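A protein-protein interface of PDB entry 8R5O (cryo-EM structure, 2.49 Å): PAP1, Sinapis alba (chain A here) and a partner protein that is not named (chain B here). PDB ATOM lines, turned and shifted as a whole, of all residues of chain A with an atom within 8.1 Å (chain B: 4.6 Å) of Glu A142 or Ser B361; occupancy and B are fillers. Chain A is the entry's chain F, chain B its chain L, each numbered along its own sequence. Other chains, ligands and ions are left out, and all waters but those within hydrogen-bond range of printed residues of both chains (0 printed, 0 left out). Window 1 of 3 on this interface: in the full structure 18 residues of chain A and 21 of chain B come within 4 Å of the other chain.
The side-chain hydroxyl (OG) of Ser B364 lies within hydrogen-bond range of the guanidinium group (NH2) of Arg A107 (3.3 Å).
The side-chain hydroxyl (OG) of Ser B364 lies within hydrogen-bond range of the side-chain carboxylate (OE2) of Glu A142 (3.3 Å).
A ring nitrogen (ND1) of His B358 is in hydrogen-bond range of the side-chain hydroxyl (OG) of Ser B361 (2.7 Å).
The side-chain carboxylate (OE2) of Glu A142 lies within salt-bridge range of the guanidinium group (NH2) of Arg A107 (2.4 Å).
O of Ser B361 lies within hydrogen-bond range of OG of Ser B364.
OG of Ser B364 lies within hydrogen-bond range of O of Asn B360, at 3.1 Å.
Met A79 touches Pro B409 (CG to O, 3.9 Å).
CD1 of Leu B481 touches NE of Arg A107 (3.98 Å).
O of Asn B360 touches OE1 of Glu A142 (3.6 Å).
Glu A142 touches Ser B361.
Ser B361 touches just one residue of chain A: Glu A142.
Of the printed residues of chain B, Met A79 touches Pro B409 (3.9 Å).
Of the printed residues of chain B, Arg A107 touches Ser B364 (3.3 Å) and Leu B481 (3.98 Å).
Met A167 touches none of the printed residues of chain B.
Tyr A172 touches none of the printed residues of chain B.
The nearest printed residue of chain B that does not touch Glu A142 is His B358 (4.7 Å).
Along chain A the printed residues that touch a printed residue of chain B span positions 79 to 142.
Hydrophobic or aromatic side chains of chain B that line the printed part of chain A: Leu B481.
Among the printed residues, 6 pairs touch across the chains.
Among the printed residues, no Asp or Glu carboxylate lies within 4 Å of a Lys or Arg side-chain nitrogen of the other chain.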
ATOM      1  N   MET A  79     -10.403  26.471  25.887  1.00  0.00           N
ATOM      2  CA  MET A  79     -10.237  27.545  24.916  1.00  0.00           C
ATOM      3  C   MET A  79      -9.541  28.764  25.504  1.00  0.00           C
ATOM      4  O   MET A  79      -9.042  29.598  24.743  1.00  0.00           O
ATOM      5  CB  MET A  79     -11.592  27.943  24.329  1.00  0.00           C
ATOM      6  CG  MET A  79     -12.087  26.991  23.255  1.00  0.00           C
ATOM      7  SD  MET A  79     -10.794  26.642  22.047  1.00  0.00           S
ATOM      8  CE  MET A  79     -11.668  25.590  20.893  1.00  0.00           C
ATOM      9  N   PRO A 106     -14.783  17.331  18.122  1.00  0.00           N
ATOM     10  CA  PRO A 106     -13.929  18.036  17.151  1.00  0.00           C
ATOM     11  C   PRO A 106     -13.457  19.397  17.627  1.00  0.00           C
ATOM     12  O   PRO A 106     -12.346  19.812  17.273  1.00  0.00           O
ATOM     13  CB  PRO A 106     -14.832  18.152  15.916  1.00  0.00           C
ATOM     14  CG  PRO A 106     -15.816  17.043  16.064  1.00  0.00           C
ATOM     15  CD  PRO A 106     -16.070  16.929  17.536  1.00  0.00           C
ATOM     16  N   ARG A 107     -14.261  20.110  18.417  1.00  0.00           N
ATOM     17  CA  ARG A 107     -13.867  21.440  18.860  1.00  0.00           C
ATOM     18  C   ARG A 107     -12.898  21.409  20.034  1.00  0.00           C
ATOM     19  O   ARG A 107     -12.261  22.428  20.316  1.00  0.00           O
ATOM     20  CB  ARG A 107     -15.103  22.262  19.232  1.00  0.00           C
ATOM     21  CG  ARG A 107     -16.169  22.289  18.151  1.00  0.00           C
ATOM     22  CD  ARG A 107     -17.016  23.547  18.222  1.00  0.00           C
ATOM     23  NE  ARG A 107     -16.650  24.506  17.187  1.00  0.00           N
ATOM     24  CZ  ARG A 107     -17.153  24.511  15.960  1.00  0.00           C
ATOM     25  NH1 ARG A 107     -18.054  23.621  15.579  1.00  0.00           N
ATOM     26  NH2 ARG A 107     -16.740  25.430  15.093  1.00  0.00           N
ATOM     27  N   HIS A 110      -9.649  20.920  18.178  1.00  0.00           N
ATOM     28  CA  HIS A 110      -9.352  22.162  17.476  1.00  0.00           C
ATOM     29  C   HIS A 110      -8.559  23.110  18.365  1.00  0.00           C
ATOM     30  O   HIS A 110      -7.618  23.765  17.905  1.00  0.00           O
ATOM     31  CB  HIS A 110     -10.648  22.820  17.005  1.00  0.00           C
ATOM     32  CG  HIS A 110     -10.451  24.159  16.365  1.00  0.00           C
ATOM     33  ND1 HIS A 110     -10.282  24.317  15.007  1.00  0.00           N
ATOM     34  CD2 HIS A 110     -10.396  25.402  16.898  1.00  0.00           C
ATOM     35  CE1 HIS A 110     -10.130  25.600  14.730  1.00  0.00           C
ATOM     36  NE2 HIS A 110     -10.195  26.279  15.860  1.00  0.00           N
ATOM     37  N   VAL A 113      -4.968  21.817  18.399  1.00  0.00           N
ATOM     38  CA  VAL A 113      -4.246  22.141  17.171  1.00  0.00           C
ATOM     39  C   VAL A 113      -3.863  23.615  17.155  1.00  0.00           C
ATOM     40  O   VAL A 113      -2.726  23.977  16.834  1.00  0.00           O
ATOM     41  CB  VAL A 113      -5.088  21.767  15.937  1.00  0.00           C
ATOM     42  CG1 VAL A 113      -4.414  22.261  14.669  1.00  0.00           C
ATOM     43  CG2 VAL A 113      -5.305  20.268  15.876  1.00  0.00           C
ATOM     44  N   VAL A 114      -4.810  24.487  17.509  1.00  0.00           N
ATOM     45  CA  VAL A 114      -4.563  25.926  17.460  1.00  0.00           C
ATOM     46  C   VAL A 114      -3.459  26.319  18.433  1.00  0.00           C
ATOM     47  O   VAL A 114      -2.591  27.138  18.107  1.00  0.00           O
ATOM     48  CB  VAL A 114      -5.867  26.698  17.737  1.00  0.00           C
ATOM     49  CG1 VAL A 114      -5.572  28.161  18.008  1.00  0.00           C
ATOM     50  CG2 VAL A 114      -6.818  26.562  16.559  1.00  0.00           C
ATOM     51  N   PRO A 139     -12.161  16.254  11.991  1.00  0.00           N
ATOM     52  CA  PRO A 139     -11.630  17.610  12.167  1.00  0.00           C
ATOM     53  C   PRO A 139     -12.490  18.652  11.468  1.00  0.00           C
ATOM     54  O   PRO A 139     -13.028  18.422  10.383  1.00  0.00           O
ATOM     55  CB  PRO A 139     -10.231  17.526  11.550  1.00  0.00           C
ATOM     56  CG  PRO A 139     -10.290  16.365  10.627  1.00  0.00           C
ATOM     57  CD  PRO A 139     -11.226  15.385  11.259  1.00  0.00           C
ATOM     58  N   LEU A 140     -12.613  19.808  12.109  1.00  0.00           N
ATOM     59  CA  LEU A 140     -13.389  20.898  11.549  1.00  0.00           C
ATOM     60  C   LEU A 140     -12.676  21.485  10.332  1.00  0.00           C
ATOM     61  O   LEU A 140     -11.453  21.388  10.216  1.00  0.00           O
ATOM     62  CB  LEU A 140     -13.606  21.981  12.601  1.00  0.00           C
ATOM     63  CG  LEU A 140     -14.319  21.543  13.881  1.00  0.00           C
ATOM     64  CD1 LEU A 140     -14.192  22.605  14.957  1.00  0.00           C
ATOM     65  CD2 LEU A 140     -15.778  21.248  13.593  1.00  0.00           C
ATOM     66  N   PRO A 141     -13.423  22.086   9.399  1.00  0.00           N
ATOM     67  CA  PRO A 141     -12.759  22.762   8.271  1.00  0.00           C
ATOM     68  C   PRO A 141     -11.810  23.854   8.721  1.00  0.00           C
ATOM     69  O   PRO A 141     -10.763  24.062   8.098  1.00  0.00           O
ATOM     70  CB  PRO A 141     -13.934  23.325   7.460  1.00  0.00           C
ATOM     71  CG  PRO A 141     -15.102  22.484   7.844  1.00  0.00           C
ATOM     72  CD  PRO A 141     -14.890  22.128   9.283  1.00  0.00           C
ATOM     73  N   GLU A 142     -12.154  24.559   9.799  1.00  0.00           N
ATOM     74  CA  GLU A 142     -11.258  25.567  10.349  1.00  0.00           C
ATOM     75  C   GLU A 142     -10.004  24.942  10.946  1.00  0.00           C
ATOM     76  O   GLU A 142      -8.936  25.561  10.923  1.00  0.00           O
ATOM     77  CB  GLU A 142     -12.001  26.394  11.396  1.00  0.00           C
ATOM     78  CG  GLU A 142     -12.754  25.552  12.412  1.00  0.00           C
ATOM     79  CD  GLU A 142     -13.896  26.304  13.067  1.00  0.00           C
ATOM     80  OE1 GLU A 142     -14.021  27.523  12.834  1.00  0.00           O
ATOM     81  OE2 GLU A 142     -14.673  25.670  13.810  1.00  0.00           O
ATOM     82  N   THR A 143     -10.115  23.727  11.489  1.00  0.00           N
ATOM     83  CA  THR A 143      -8.944  23.057  12.045  1.00  0.00           C
ATOM     84  C   THR A 143      -7.920  22.750  10.962  1.00  0.00           C
ATOM     85  O   THR A 143      -6.713  22.926  11.171  1.00  0.00           O
ATOM     86  CB  THR A 143      -9.361  21.774  12.763  1.00  0.00           C
ATOM     87  OG1 THR A 143     -10.347  22.081  13.757  1.00  0.00           O
ATOM     88  CG2 THR A 143      -8.161  21.129  13.435  1.00  0.00           C
ATOM     89  N   MET A 144      -8.382  22.289   9.798  1.00  0.00           N
ATOM     90  CA  MET A 144      -7.469  22.005   8.698  1.00  0.00           C
ATOM     91  C   MET A 144      -6.833  23.283   8.165  1.00  0.00           C
ATOM     92  O   MET A 144      -5.655  23.288   7.792  1.00  0.00           O
ATOM     93  CB  MET A 144      -8.208  21.268   7.583  1.00  0.00           C
ATOM     94  CG  MET A 144      -8.982  20.046   8.052  1.00  0.00           C
ATOM     95  SD  MET A 144      -7.945  18.812   8.863  1.00  0.00           S
ATOM     96  CE  MET A 144      -6.884  18.304   7.516  1.00  0.00           C
ATOM     97  N   ILE A 145      -7.595  24.377   8.127  1.00  0.00           N
ATOM     98  CA  ILE A 145      -7.063  25.647   7.645  1.00  0.00           C
ATOM     99  C   ILE A 145      -5.961  26.160   8.565  1.00  0.00           C
ATOM    100  O   ILE A 145      -4.986  26.764   8.100  1.00  0.00           O
ATOM    101  CB  ILE A 145      -8.205  26.667   7.490  1.00  0.00           C
ATOM    102  CG1 ILE A 145      -9.135  26.244   6.353  1.00  0.00           C
ATOM    103  CG2 ILE A 145      -7.664  28.056   7.223  1.00  0.00           C
ATOM    104  CD1 ILE A 145     -10.271  27.202   6.109  1.00  0.00           C
ATOM    105  N   ALA A 146      -6.083  25.923   9.873  1.00  0.00           N
ATOM    106  CA  ALA A 146      -5.025  26.321  10.795  1.00  0.00           C
ATOM    107  C   ALA A 146      -3.744  25.537  10.536  1.00  0.00           C
ATOM    108  O   ALA A 146      -2.641  26.081  10.657  1.00  0.00           O
ATOM    109  CB  ALA A 146      -5.485  26.134  12.239  1.00  0.00           C
ATOM    110  N   LEU A 147      -3.872  24.258  10.183  1.00  0.00           N
ATOM    111  CA  LEU A 147      -2.697  23.458   9.855  1.00  0.00           C
ATOM    112  C   LEU A 147      -2.121  23.847   8.498  1.00  0.00           C
ATOM    113  O   LEU A 147      -0.898  23.883   8.325  1.00  0.00           O
ATOM    114  CB  LEU A 147      -3.054  21.973   9.882  1.00  0.00           C
ATOM    115  CG  LEU A 147      -3.254  21.353  11.263  1.00  0.00           C
ATOM    116  CD1 LEU A 147      -3.965  20.020  11.153  1.00  0.00           C
ATOM    117  CD2 LEU A 147      -1.914  21.183  11.950  1.00  0.00           C
ATOM    118  N   VAL A 148      -2.986  24.131   7.521  1.00  0.00           N
ATOM    119  CA  VAL A 148      -2.517  24.522   6.194  1.00  0.00           C
ATOM    120  C   VAL A 148      -1.778  25.852   6.261  1.00  0.00           C
ATOM    121  O   VAL A 148      -0.696  26.013   5.685  1.00  0.00           O
ATOM    122  CB  VAL A 148      -3.694  24.577   5.203  1.00  0.00           C
ATOM    123  CG1 VAL A 148      -3.279  25.270   3.918  1.00  0.00           C
ATOM    124  CG2 VAL A 148      -4.196  23.178   4.909  1.00  0.00           C
ATOM    125  N   ARG A 149      -2.350  26.826   6.972  1.00  0.00           N
ATOM    126  CA  ARG A 149      -1.691  28.121   7.112  1.00  0.00           C
ATOM    127  C   ARG A 149      -0.377  27.999   7.872  1.00  0.00           C
ATOM    128  O   ARG A 149       0.595  28.692   7.547  1.00  0.00           O
ATOM    129  CB  ARG A 149      -2.633  29.117   7.797  1.00  0.00           C
ATOM    130  CG  ARG A 149      -1.927  30.267   8.495  1.00  0.00           C
ATOM    131  CD  ARG A 149      -2.858  31.437   8.773  1.00  0.00           C
ATOM    132  NE  ARG A 149      -4.200  31.012   9.149  1.00  0.00           N
ATOM    133  CZ  ARG A 149      -5.293  31.280   8.448  1.00  0.00           C
ATOM    134  NH1 ARG A 149      -5.244  32.000   7.340  1.00  0.00           N
ATOM    135  NH2 ARG A 149      -6.466  30.822   8.875  1.00  0.00           N
ATOM    136  N   MET A 167      -8.528  17.483   3.152  1.00  0.00           N
ATOM    137  CA  MET A 167      -9.780  18.235   3.144  1.00  0.00           C
ATOM    138  C   MET A 167     -10.680  17.799   1.995  1.00  0.00           C
ATOM    139  O   MET A 167     -11.902  17.698   2.157  1.00  0.00           O
ATOM    140  CB  MET A 167      -9.497  19.733   3.057  1.00  0.00           C
ATOM    141  CG  MET A 167      -8.594  20.254   4.155  1.00  0.00           C
ATOM    142  SD  MET A 167      -8.335  22.034   4.070  1.00  0.00           S
ATOM    143  CE  MET A 167      -9.992  22.628   4.389  1.00  0.00           C
ATOM    144  N   TYR A 172     -14.522  18.568   2.240  1.00  0.00           N
ATOM    145  CA  TYR A 172     -14.589  20.001   2.477  1.00  0.00           C
ATOM    146  C   TYR A 172     -14.346  20.759   1.174  1.00  0.00           C
ATOM    147  O   TYR A 172     -14.160  20.172   0.104  1.00  0.00           O
ATOM    148  CB  TYR A 172     -13.582  20.416   3.546  1.00  0.00           C
ATOM    149  CG  TYR A 172     -13.915  19.929   4.937  1.00  0.00           C
ATOM    150  CD1 TYR A 172     -15.224  19.647   5.300  1.00  0.00           C
ATOM    151  CD2 TYR A 172     -12.920  19.753   5.887  1.00  0.00           C
ATOM    152  CE1 TYR A 172     -15.531  19.201   6.571  1.00  0.00           C
ATOM    153  CE2 TYR A 172     -13.217  19.309   7.158  1.00  0.00           C
ATOM    154  CZ  TYR A 172     -14.523  19.034   7.495  1.00  0.00           C
ATOM    155  OH  TYR A 172     -14.824  18.591   8.763  1.00  0.00           O
ATOM    156  N   GLN A 176     -10.734  27.889  -0.411  1.00  0.00           N
ATOM    157  CA  GLN A 176     -10.316  28.913   0.540  1.00  0.00           C
ATOM    158  C   GLN A 176      -8.999  28.544   1.212  1.00  0.00           C
ATOM    159  O   GLN A 176      -8.146  29.410   1.435  1.00  0.00           O
ATOM    160  CB  GLN A 176     -11.410  29.141   1.580  1.00  0.00           C
ATOM    161  CG  GLN A 176     -11.034  30.137   2.661  1.00  0.00           C
ATOM    162  CD  GLN A 176     -12.213  30.527   3.525  1.00  0.00           C
ATOM    163  OE1 GLN A 176     -13.343  30.618   3.048  1.00  0.00           O
ATOM    164  NE2 GLN A 176     -11.956  30.758   4.807  1.00  0.00           N
ATOM    165  N   HIS B 358     -18.440  34.755  16.375  1.00  0.00           N
ATOM    166  CA  HIS B 358     -17.276  34.310  15.619  1.00  0.00           C
ATOM    167  C   HIS B 358     -17.732  33.917  14.219  1.00  0.00           C
ATOM    168  O   HIS B 358     -18.499  32.963  14.054  1.00  0.00           O
ATOM    169  CB  HIS B 358     -16.590  33.150  16.334  1.00  0.00           C
ATOM    170  CG  HIS B 358     -15.206  32.867  15.842  1.00  0.00           C
ATOM    171  ND1 HIS B 358     -14.880  31.715  15.162  1.00  0.00           N
ATOM    172  CD2 HIS B 358     -14.063  33.585  15.935  1.00  0.00           C
ATOM    173  CE1 HIS B 358     -13.596  31.735  14.857  1.00  0.00           C
ATOM    174  NE2 HIS B 358     -13.076  32.859  15.316  1.00  0.00           N
ATOM    175  N   LEU B 359     -17.260  34.654  13.210  1.00  0.00           N
ATOM    176  CA  LEU B 359     -17.695  34.400  11.840  1.00  0.00           C
ATOM    177  C   LEU B 359     -17.302  33.003  11.381  1.00  0.00           C
ATOM    178  O   LEU B 359     -18.103  32.305  10.749  1.00  0.00           O
ATOM    179  CB  LEU B 359     -17.114  35.453  10.897  1.00  0.00           C
ATOM    180  CG  LEU B 359     -17.431  35.258   9.411  1.00  0.00           C
ATOM    181  CD1 LEU B 359     -18.933  35.158   9.180  1.00  0.00           C
ATOM    182  CD2 LEU B 359     -16.835  36.382   8.581  1.00  0.00           C
ATOM    183  N   ASN B 360     -16.077  32.574  11.689  1.00  0.00           N
ATOM    184  CA  ASN B 360     -15.622  31.264  11.234  1.00  0.00           C
ATOM    185  C   ASN B 360     -16.447  30.145  11.854  1.00  0.00           C
ATOM    186  O   ASN B 360     -16.807  29.180  11.172  1.00  0.00           O
ATOM    187  CB  ASN B 360     -14.141  31.078  11.557  1.00  0.00           C
ATOM    188  CG  ASN B 360     -13.270  32.134  10.915  1.00  0.00           C
ATOM    189  OD1 ASN B 360     -13.729  33.233  10.614  1.00  0.00           O
ATOM    190  ND2 ASN B 360     -12.002  31.806  10.702  1.00  0.00           N
ATOM    191  N   SER B 361     -16.750  30.255  13.150  1.00  0.00           N
ATOM    192  CA  SER B 361     -17.555  29.237  13.817  1.00  0.00           C
ATOM    193  C   SER B 361     -18.964  29.184  13.241  1.00  0.00           C
ATOM    194  O   SER B 361     -19.494  28.101  12.969  1.00  0.00           O
ATOM    195  CB  SER B 361     -17.596  29.507  15.320  1.00  0.00           C
ATOM    196  OG  SER B 361     -16.295  29.516  15.875  1.00  0.00           O
ATOM    197  N   PHE B 362     -19.586  30.350  13.047  1.00  0.00           N
ATOM    198  CA  PHE B 362     -20.943  30.392  12.513  1.00  0.00           C
ATOM    199  C   PHE B 362     -21.015  29.756  11.131  1.00  0.00           C
ATOM    200  O   PHE B 362     -21.955  29.013  10.829  1.00  0.00           O
ATOM    201  CB  PHE B 362     -21.442  31.836  12.468  1.00  0.00           C
ATOM    202  CG  PHE B 362     -22.894  31.968  12.104  1.00  0.00           C
ATOM    203  CD1 PHE B 362     -23.284  32.115  10.783  1.00  0.00           C
ATOM    204  CD2 PHE B 362     -23.870  31.948  13.086  1.00  0.00           C
ATOM    205  CE1 PHE B 362     -24.619  32.237  10.449  1.00  0.00           C
ATOM    206  CE2 PHE B 362     -25.204  32.072  12.759  1.00  0.00           C
ATOM    207  CZ  PHE B 362     -25.579  32.216  11.438  1.00  0.00           C
ATOM    208  N   LEU B 363     -20.030  30.037  10.276  1.00  0.00           N
ATOM    209  CA  LEU B 363     -20.024  29.460   8.935  1.00  0.00           C
ATOM    210  C   LEU B 363     -19.831  27.950   8.978  1.00  0.00           C
ATOM    211  O   LEU B 363     -20.476  27.216   8.220  1.00  0.00           O
ATOM    212  CB  LEU B 363     -18.935  30.113   8.088  1.00  0.00           C
ATOM    213  CG  LEU B 363     -19.097  31.604   7.798  1.00  0.00           C
ATOM    214  CD1 LEU B 363     -17.876  32.144   7.078  1.00  0.00           C
ATOM    215  CD2 LEU B 363     -20.355  31.854   6.987  1.00  0.00           C
ATOM    216  N   SER B 364     -18.945  27.467   9.851  1.00  0.00           N
ATOM    217  CA  SER B 364     -18.662  26.038   9.914  1.00  0.00           C
ATOM    218  C   SER B 364     -19.782  25.258  10.588  1.00  0.00           C
ATOM    219  O   SER B 364     -20.014  24.095  10.242  1.00  0.00           O
ATOM    220  CB  SER B 364     -17.345  25.794  10.651  1.00  0.00           C
ATOM    221  OG  SER B 364     -17.414  26.267  11.984  1.00  0.00           O
ATOM    222  N   VAL B 365     -20.472  25.871  11.552  1.00  0.00           N
ATOM    223  CA  VAL B 365     -21.590  25.204  12.211  1.00  0.00           C
ATOM    224  C   VAL B 365     -22.686  24.877  11.205  1.00  0.00           C
ATOM    225  O   VAL B 365     -23.268  23.786  11.230  1.00  0.00           O
ATOM    226  CB  VAL B 365     -22.117  26.075  13.367  1.00  0.00           C
ATOM    227  CG1 VAL B 365     -23.587  25.804  13.622  1.00  0.00           C
ATOM    228  CG2 VAL B 365     -21.304  25.822  14.624  1.00  0.00           C
ATOM    229  N   PRO B 409     -12.889  31.048  19.585  1.00  0.00           N
ATOM    230  CA  PRO B 409     -13.780  31.820  20.457  1.00  0.00           C
ATOM    231  C   PRO B 409     -14.037  31.140  21.793  1.00  0.00           C
ATOM    232  O   PRO B 409     -14.213  29.923  21.881  1.00  0.00           O
ATOM    233  CB  PRO B 409     -15.069  31.902  19.631  1.00  0.00           C
ATOM    234  CG  PRO B 409     -15.079  30.627  18.862  1.00  0.00           C
ATOM    235  CD  PRO B 409     -13.636  30.295  18.561  1.00  0.00           C
ATOM    236  N   TYR B 477     -26.397  27.793  16.758  1.00  0.00           N
ATOM    237  CA  TYR B 477     -24.967  28.077  16.784  1.00  0.00           C
ATOM    238  C   TYR B 477     -24.426  28.079  18.208  1.00  0.00           C
ATOM    239  O   TYR B 477     -23.333  27.563  18.466  1.00  0.00           O
ATOM    240  CB  TYR B 477     -24.693  29.418  16.104  1.00  0.00           C
ATOM    241  CG  TYR B 477     -23.382  30.057  16.490  1.00  0.00           C
ATOM    242  CD1 TYR B 477     -22.191  29.651  15.908  1.00  0.00           C
ATOM    243  CD2 TYR B 477     -23.335  31.077  17.430  1.00  0.00           C
ATOM    244  CE1 TYR B 477     -20.991  30.237  16.255  1.00  0.00           C
ATOM    245  CE2 TYR B 477     -22.140  31.665  17.785  1.00  0.00           C
ATOM    246  CZ  TYR B 477     -20.972  31.242  17.194  1.00  0.00           C
ATOM    247  OH  TYR B 477     -19.779  31.826  17.544  1.00  0.00           O
ATOM    248  N   LEU B 481     -21.544  25.024  19.610  1.00  0.00           N
ATOM    249  CA  LEU B 481     -20.216  25.507  19.965  1.00  0.00           C
ATOM    250  C   LEU B 481     -19.667  24.827  21.214  1.00  0.00           C
ATOM    251  O   LEU B 481     -18.838  25.413  21.923  1.00  0.00           O
ATOM    252  CB  LEU B 481     -20.245  27.023  20.153  1.00  0.00           C
ATOM    253  CG  LEU B 481     -19.108  27.794  19.487  1.00  0.00           C
ATOM    254  CD1 LEU B 481     -19.115  27.527  17.993  1.00  0.00           C
ATOM    255  CD2 LEU B 481     -19.234  29.279  19.772  1.00  0.00           C
